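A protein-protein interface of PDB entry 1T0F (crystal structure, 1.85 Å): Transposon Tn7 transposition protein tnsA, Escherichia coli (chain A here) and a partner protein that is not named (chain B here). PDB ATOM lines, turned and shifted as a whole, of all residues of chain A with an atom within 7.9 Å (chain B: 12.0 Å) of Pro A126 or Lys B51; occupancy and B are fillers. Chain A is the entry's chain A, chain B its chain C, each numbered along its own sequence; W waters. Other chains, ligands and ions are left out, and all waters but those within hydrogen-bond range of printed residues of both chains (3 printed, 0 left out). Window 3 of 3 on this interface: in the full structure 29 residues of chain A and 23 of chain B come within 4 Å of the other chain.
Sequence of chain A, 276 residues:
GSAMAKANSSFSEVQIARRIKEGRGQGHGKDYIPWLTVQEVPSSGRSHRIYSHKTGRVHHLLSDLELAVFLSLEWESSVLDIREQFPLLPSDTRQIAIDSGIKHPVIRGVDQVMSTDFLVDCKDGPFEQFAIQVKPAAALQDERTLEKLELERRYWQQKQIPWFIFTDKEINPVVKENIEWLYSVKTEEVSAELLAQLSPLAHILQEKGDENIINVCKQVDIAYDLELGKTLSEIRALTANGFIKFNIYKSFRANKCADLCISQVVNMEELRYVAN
No residue of chain B comes within 4 Å of Asp A124. Of the printed residues of chain B, Pro A126 touches Leu B49, Phe B50 and Lys B51. Printed residues of chain B within 4 Å of Phe A127: Leu B49 (3.7 Å). No residue of chain B comes within 4 Å of Glu A128. Printed residues of chain B within 4 Å of Phe A130: Leu B49 (3.7 Å) and Phe B50 (3.6 Å). Printed residues of chain A within 4 Å of Phe B50: Glu A76, Ser A78, Cys A122, Pro A126 and Phe A130. Of chain A, only Pro A126 (3.9 Å) comes within 4 Å of Lys B51. The nearest residue of chain A that does not touch Lys B51 is Glu A76 (5.2 Å).
The side-chain sulfur (SG) of Cys A122 sits close to the backbone carbonyl oxygen (O) of Phe A127 (3.5 Å). N of Cys A122 is in hydrogen-bond range of O of Glu A128, 2.8 Å away.
Water W1 lies within hydrogen-bond range of the backbone carbonyl oxygen (O) of Lys B51 and the side-chain carboxylate (OE1) of Glu A76. Water W2 lies within hydrogen-bond range of O of Leu B49, O of Phe A127 and SG of Cys A122. Water W3 lies within hydrogen-bond range of the side-chain hydroxyl of Ser A78 (3.1 Å) and the backbone NH of Lys B51 (3.1 Å).
Of the 13 printed residues of chain A, 6 touch a printed residue of chain B. Printed residues of chain A that touch a printed residue of chain B: Glu A76, Ser A78, Cys A122, Pro A126, Phe A127 and Phe A130. Among the printed residues, 9 pairs touch across the chains. Among the printed residues, no Asp or Glu carboxylate lies within 4 Å of a Lys or Arg side-chain nitrogen of the other chain.
CB of Phe B50 touches OE1 of Glu A76, at 3.4 Å. Phe B50 touches Ser A78 (CD2 to OG, 3.3 Å). Phe B50 touches Cys A122. Pro A126 touches Leu B49. Pro A126 touches Phe B50. CD of Pro A126 touches N of Lys B51, at 3.9 Å. CD2 of Leu B49 touches CE2 of Phe A127, 3.7 Å away. Phe A130 touches Leu B49. Phe A130 touches Phe B50.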
ATOM      1  N   TRP A  75     -14.868  26.194 -14.602  1.00  0.00           N
ATOM      2  CA  TRP A  75     -14.627  24.851 -15.128  1.00  0.00           C
ATOM      3  C   TRP A  75     -15.886  23.970 -15.053  1.00  0.00           C
ATOM      4  O   TRP A  75     -16.099  23.115 -15.912  1.00  0.00           O
ATOM      5  CB  TRP A  75     -13.503  24.183 -14.335  1.00  0.00           C
ATOM      6  CG  TRP A  75     -13.246  22.755 -14.728  1.00  0.00           C
ATOM      7  CD1 TRP A  75     -12.473  22.314 -15.765  1.00  0.00           C
ATOM      8  CD2 TRP A  75     -13.791  21.586 -14.107  1.00  0.00           C
ATOM      9  NE1 TRP A  75     -12.501  20.938 -15.825  1.00  0.00           N
ATOM     10  CE2 TRP A  75     -13.304  20.467 -14.820  1.00  0.00           C
ATOM     11  CE3 TRP A  75     -14.647  21.376 -13.018  1.00  0.00           C
ATOM     12  CZ2 TRP A  75     -13.645  19.155 -14.478  1.00  0.00           C
ATOM     13  CZ3 TRP A  75     -14.987  20.068 -12.676  1.00  0.00           C
ATOM     14  CH2 TRP A  75     -14.484  18.975 -13.406  1.00  0.00           C
ATOM     15  N   GLU A  76     -16.706  24.170 -14.021  1.00  0.00           N
ATOM     16  CA  GLU A  76     -17.927  23.377 -13.821  1.00  0.00           C
ATOM     17  C   GLU A  76     -18.978  23.578 -14.909  1.00  0.00           C
ATOM     18  O   GLU A  76     -19.437  24.694 -15.138  1.00  0.00           O
ATOM     19  CB  GLU A  76     -18.552  23.707 -12.463  1.00  0.00           C
ATOM     20  CG  GLU A  76     -17.697  23.328 -11.259  1.00  0.00           C
ATOM     21  CD  GLU A  76     -17.572  21.823 -11.067  1.00  0.00           C
ATOM     22  OE1 GLU A  76     -18.393  21.072 -11.641  1.00  0.00           O
ATOM     23  OE2 GLU A  76     -16.662  21.395 -10.324  1.00  0.00           O
ATOM     24  N   SER A  77     -19.391  22.492 -15.559  1.00  0.00           N
ATOM     25  CA  SER A  77     -20.378  22.611 -16.631  1.00  0.00           C
ATOM     26  C   SER A  77     -21.737  23.170 -16.198  1.00  0.00           C
ATOM     27  O   SER A  77     -22.381  23.881 -16.963  1.00  0.00           O
ATOM     28  CB  SER A  77     -20.584  21.256 -17.321  1.00  0.00           C
ATOM     29  OG  SER A  77     -21.218  20.328 -16.463  1.00  0.00           O
ATOM     30  N   SER A  78     -22.161  22.870 -14.976  1.00  0.00           N
ATOM     31  CA  SER A  78     -23.462  23.323 -14.482  1.00  0.00           C
ATOM     32  C   SER A  78     -23.575  24.800 -14.086  1.00  0.00           C
ATOM     33  O   SER A  78     -24.681  25.322 -13.963  1.00  0.00           O
ATOM     34  CB  SER A  78     -23.890  22.470 -13.291  1.00  0.00           C
ATOM     35  OG  SER A  78     -23.019  22.684 -12.194  1.00  0.00           O
ATOM     36  N   CYS A 122     -26.505  27.944 -10.707  1.00  0.00           N
ATOM     37  CA  CYS A 122     -26.246  26.726 -11.474  1.00  0.00           C
ATOM     38  C   CYS A 122     -27.518  26.282 -12.197  1.00  0.00           C
ATOM     39  O   CYS A 122     -28.631  26.543 -11.728  1.00  0.00           O
ATOM     40  CB  CYS A 122     -25.756  25.609 -10.549  1.00  0.00           C
ATOM     41  SG  CYS A 122     -24.208  25.993  -9.670  1.00  0.00           S
ATOM     42  N   ASP A 124     -28.432  23.115 -12.850  1.00  0.00           N
ATOM     43  CA  ASP A 124     -28.978  21.945 -12.177  1.00  0.00           C
ATOM     44  C   ASP A 124     -27.945  21.494 -11.164  1.00  0.00           C
ATOM     45  O   ASP A 124     -27.016  22.236 -10.855  1.00  0.00           O
ATOM     46  CB  ASP A 124     -29.245  20.810 -13.174  1.00  0.00           C
ATOM     47  CG  ASP A 124     -28.043  20.506 -14.048  1.00  0.00           C
ATOM     48  OD1 ASP A 124     -26.901  20.700 -13.584  1.00  0.00           O
ATOM     49  OD2 ASP A 124     -28.243  20.061 -15.199  1.00  0.00           O
ATOM     50  N   GLY A 125     -28.096  20.279 -10.657  1.00  0.00           N
ATOM     51  CA  GLY A 125     -27.139  19.787  -9.684  1.00  0.00           C
ATOM     52  C   GLY A 125     -27.572  20.035  -8.248  1.00  0.00           C
ATOM     53  O   GLY A 125     -28.682  20.512  -8.003  1.00  0.00           O
ATOM     54  N   PRO A 126     -26.698  19.736  -7.273  1.00  0.00           N
ATOM     55  CA  PRO A 126     -26.957  19.904  -5.838  1.00  0.00           C
ATOM     56  C   PRO A 126     -27.439  21.274  -5.361  1.00  0.00           C
ATOM     57  O   PRO A 126     -28.381  21.349  -4.582  1.00  0.00           O
ATOM     58  CB  PRO A 126     -25.629  19.499  -5.194  1.00  0.00           C
ATOM     59  CG  PRO A 126     -24.627  19.821  -6.249  1.00  0.00           C
ATOM     60  CD  PRO A 126     -25.303  19.319  -7.499  1.00  0.00           C
ATOM     61  N   PHE A 127     -26.798  22.343  -5.824  1.00  0.00           N
ATOM     62  CA  PHE A 127     -27.163  23.705  -5.420  1.00  0.00           C
ATOM     63  C   PHE A 127     -27.491  24.598  -6.612  1.00  0.00           C
ATOM     64  O   PHE A 127     -26.636  24.838  -7.458  1.00  0.00           O
ATOM     65  CB  PHE A 127     -26.007  24.344  -4.637  1.00  0.00           C
ATOM     66  CG  PHE A 127     -25.652  23.609  -3.379  1.00  0.00           C
ATOM     67  CD1 PHE A 127     -26.414  23.772  -2.225  1.00  0.00           C
ATOM     68  CD2 PHE A 127     -24.578  22.728  -3.354  1.00  0.00           C
ATOM     69  CE1 PHE A 127     -26.107  23.063  -1.063  1.00  0.00           C
ATOM     70  CE2 PHE A 127     -24.265  22.018  -2.203  1.00  0.00           C
ATOM     71  CZ  PHE A 127     -25.032  22.185  -1.053  1.00  0.00           C
ATOM     72  N   GLU A 128     -28.720  25.107  -6.665  1.00  0.00           N
ATOM     73  CA  GLU A 128     -29.129  25.977  -7.762  1.00  0.00           C
ATOM     74  C   GLU A 128     -28.523  27.371  -7.573  1.00  0.00           C
ATOM     75  O   GLU A 128     -28.332  28.124  -8.530  1.00  0.00           O
ATOM     76  CB  GLU A 128     -30.655  26.055  -7.830  1.00  0.00           C
ATOM     77  CG  GLU A 128     -31.326  26.862  -6.726  1.00  0.00           C
ATOM     78  CD  GLU A 128     -32.841  26.671  -6.708  1.00  0.00           C
ATOM     79  OE1 GLU A 128     -33.435  26.518  -7.801  1.00  0.00           O
ATOM     80  OE2 GLU A 128     -33.439  26.683  -5.605  1.00  0.00           O
ATOM     81  N   GLN A 129     -28.215  27.702  -6.327  1.00  0.00           N
ATOM     82  CA  GLN A 129     -27.601  28.981  -6.019  1.00  0.00           C
ATOM     83  C   GLN A 129     -26.853  28.856  -4.702  1.00  0.00           C
ATOM     84  O   GLN A 129     -27.343  28.240  -3.758  1.00  0.00           O
ATOM     85  CB  GLN A 129     -28.668  30.069  -5.901  1.00  0.00           C
ATOM     86  CG  GLN A 129     -28.139  31.484  -6.074  1.00  0.00           C
ATOM     87  CD  GLN A 129     -29.255  32.515  -6.160  1.00  0.00           C
ATOM     88  OE1 GLN A 129     -29.106  33.558  -6.798  1.00  0.00           O
ATOM     89  NE2 GLN A 129     -30.377  32.227  -5.512  1.00  0.00           N
ATOM     90  N   PHE A 130     -25.651  29.410  -4.646  1.00  0.00           N
ATOM     91  CA  PHE A 130     -24.895  29.377  -3.405  1.00  0.00           C
ATOM     92  C   PHE A 130     -23.934  30.540  -3.395  1.00  0.00           C
ATOM     93  O   PHE A 130     -23.596  31.081  -4.444  1.00  0.00           O
ATOM     94  CB  PHE A 130     -24.161  28.036  -3.214  1.00  0.00           C
ATOM     95  CG  PHE A 130     -23.122  27.735  -4.258  1.00  0.00           C
ATOM     96  CD1 PHE A 130     -21.841  28.279  -4.168  1.00  0.00           C
ATOM     97  CD2 PHE A 130     -23.412  26.876  -5.318  1.00  0.00           C
ATOM     98  CE1 PHE A 130     -20.861  27.975  -5.110  1.00  0.00           C
ATOM     99  CE2 PHE A 130     -22.440  26.562  -6.268  1.00  0.00           C
ATOM    100  CZ  PHE A 130     -21.159  27.114  -6.164  1.00  0.00           C
ATOM    101  N   PRO A 162     -27.563  28.900   0.537  1.00  0.00           N
ATOM    102  CA  PRO A 162     -26.371  28.269   1.117  1.00  0.00           C
ATOM    103  C   PRO A 162     -25.141  29.159   0.977  1.00  0.00           C
ATOM    104  O   PRO A 162     -24.893  29.735  -0.085  1.00  0.00           O
ATOM    105  CB  PRO A 162     -26.228  26.975   0.311  1.00  0.00           C
ATOM    106  CG  PRO A 162     -27.644  26.668  -0.097  1.00  0.00           C
ATOM    107  CD  PRO A 162     -28.171  28.034  -0.489  1.00  0.00           C
ATOM    108  N   VAL B  44     -15.985  24.121   2.610  1.00  0.00           N
ATOM    109  CA  VAL B  44     -16.075  22.950   1.742  1.00  0.00           C
ATOM    110  C   VAL B  44     -15.173  23.144   0.529  1.00  0.00           C
ATOM    111  O   VAL B  44     -14.790  24.266   0.210  1.00  0.00           O
ATOM    112  CB  VAL B  44     -17.525  22.726   1.221  1.00  0.00           C
ATOM    113  CG1 VAL B  44     -18.494  22.539   2.383  1.00  0.00           C
ATOM    114  CG2 VAL B  44     -17.949  23.902   0.356  1.00  0.00           C
ATOM    115  N   ASP B  45     -14.815  22.057  -0.140  1.00  0.00           N
ATOM    116  CA  ASP B  45     -14.010  22.192  -1.349  1.00  0.00           C
ATOM    117  C   ASP B  45     -14.983  22.117  -2.517  1.00  0.00           C
ATOM    118  O   ASP B  45     -16.090  21.590  -2.380  1.00  0.00           O
ATOM    119  CB  ASP B  45     -12.937  21.100  -1.452  1.00  0.00           C
ATOM    120  CG  ASP B  45     -13.483  19.716  -1.205  1.00  0.00           C
ATOM    121  OD1 ASP B  45     -14.490  19.351  -1.845  1.00  0.00           O
ATOM    122  OD2 ASP B  45     -12.899  18.991  -0.370  1.00  0.00           O
ATOM    123  N   MET B  46     -14.569  22.651  -3.658  1.00  0.00           N
ATOM    124  CA  MET B  46     -15.408  22.693  -4.846  1.00  0.00           C
ATOM    125  C   MET B  46     -16.161  21.404  -5.154  1.00  0.00           C
ATOM    126  O   MET B  46     -17.342  21.442  -5.495  1.00  0.00           O
ATOM    127  CB  MET B  46     -14.563  23.102  -6.053  1.00  0.00           C
ATOM    128  CG  MET B  46     -15.313  23.959  -7.043  1.00  0.00           C
ATOM    129  SD  MET B  46     -16.074  25.362  -6.224  1.00  0.00           S
ATOM    130  CE  MET B  46     -14.681  26.474  -6.079  1.00  0.00           C
ATOM    131  N   ALA B  47     -15.486  20.267  -5.035  1.00  0.00           N
ATOM    132  CA  ALA B  47     -16.112  18.975  -5.315  1.00  0.00           C
ATOM    133  C   ALA B  47     -17.471  18.790  -4.630  1.00  0.00           C
ATOM    134  O   ALA B  47     -18.453  18.397  -5.268  1.00  0.00           O
ATOM    135  CB  ALA B  47     -15.174  17.849  -4.902  1.00  0.00           C
ATOM    136  N   SER B  48     -17.524  19.083  -3.333  1.00  0.00           N
ATOM    137  CA  SER B  48     -18.748  18.924  -2.557  1.00  0.00           C
ATOM    138  C   SER B  48     -19.949  19.707  -3.076  1.00  0.00           C
ATOM    139  O   SER B  48     -21.095  19.346  -2.801  1.00  0.00           O
ATOM    140  CB  SER B  48     -18.490  19.315  -1.100  1.00  0.00           C
ATOM    141  OG  SER B  48     -17.463  18.525  -0.533  1.00  0.00           O
ATOM    142  N   LEU B  49     -19.698  20.771  -3.828  1.00  0.00           N
ATOM    143  CA  LEU B  49     -20.787  21.600  -4.340  1.00  0.00           C
ATOM    144  C   LEU B  49     -21.307  21.203  -5.714  1.00  0.00           C
ATOM    145  O   LEU B  49     -22.328  21.729  -6.167  1.00  0.00           O
ATOM    146  CB  LEU B  49     -20.346  23.057  -4.394  1.00  0.00           C
ATOM    147  CG  LEU B  49     -19.844  23.662  -3.088  1.00  0.00           C
ATOM    148  CD1 LEU B  49     -19.342  25.071  -3.361  1.00  0.00           C
ATOM    149  CD2 LEU B  49     -20.958  23.657  -2.055  1.00  0.00           C
ATOM    150  N   PHE B  50     -20.612  20.290  -6.384  1.00  0.00           N
ATOM    151  CA  PHE B  50     -21.049  19.875  -7.708  1.00  0.00           C
ATOM    152  C   PHE B  50     -21.156  18.368  -7.900  1.00  0.00           C
ATOM    153  O   PHE B  50     -20.548  17.592  -7.167  1.00  0.00           O
ATOM    154  CB  PHE B  50     -20.118  20.462  -8.765  1.00  0.00           C
ATOM    155  CG  PHE B  50     -20.098  21.954  -8.773  1.00  0.00           C
ATOM    156  CD1 PHE B  50     -19.212  22.657  -7.963  1.00  0.00           C
ATOM    157  CD2 PHE B  50     -20.999  22.665  -9.563  1.00  0.00           C
ATOM    158  CE1 PHE B  50     -19.222  24.053  -7.939  1.00  0.00           C
ATOM    159  CE2 PHE B  50     -21.016  24.059  -9.546  1.00  0.00           C
ATOM    160  CZ  PHE B  50     -20.127  24.752  -8.733  1.00  0.00           C
ATOM    161  N   LYS B  51     -21.946  17.969  -8.895  1.00  0.00           N
ATOM    162  CA  LYS B  51     -22.146  16.560  -9.209  1.00  0.00           C
ATOM    163  C   LYS B  51     -20.796  15.881  -9.387  1.00  0.00           C
ATOM    164  O   LYS B  51     -19.926  16.387 -10.095  1.00  0.00           O
ATOM    165  CB  LYS B  51     -22.958  16.413 -10.498  1.00  0.00           C
ATOM    166  CG  LYS B  51     -23.144  14.970 -10.950  1.00  0.00           C
ATOM    167  CD  LYS B  51     -22.798  14.796 -12.426  1.00  0.00           C
ATOM    168  CE  LYS B  51     -23.696  15.632 -13.322  1.00  0.00           C
ATOM    169  NZ  LYS B  51     -23.340  15.488 -14.762  1.00  0.00           N
ATOM    170  N   GLN B  52     -20.626  14.735  -8.739  1.00  0.00           N
ATOM    171  CA  GLN B  52     -19.376  13.994  -8.838  1.00  0.00           C
ATOM    172  C   GLN B  52     -19.217  13.440 -10.249  1.00  0.00           C
ATOM    173  O   GLN B  52     -18.262  13.858 -10.940  1.00  0.00           O
ATOM    174  CB  GLN B  52     -19.361  12.848  -7.826  1.00  0.00           C
ATOM    175  CG  GLN B  52     -19.645  13.279  -6.394  1.00  0.00           C
ATOM    176  CD  GLN B  52     -19.517  12.133  -5.406  1.00  0.00           C
ATOM    177  OE1 GLN B  52     -20.140  11.083  -5.571  1.00  0.00           O
ATOM    178  NE2 GLN B  52     -18.709  12.333  -4.369  1.00  0.00           N
HETATM  179  O   HOH W   1     -18.209  18.180 -11.275  1.00  0.00           O
HETATM  180  O   HOH W   2     -24.442  23.011  -7.531  1.00  0.00           O
HETATM  181  O   HOH W   3     -23.274  19.875 -10.953  1.00  0.00           O
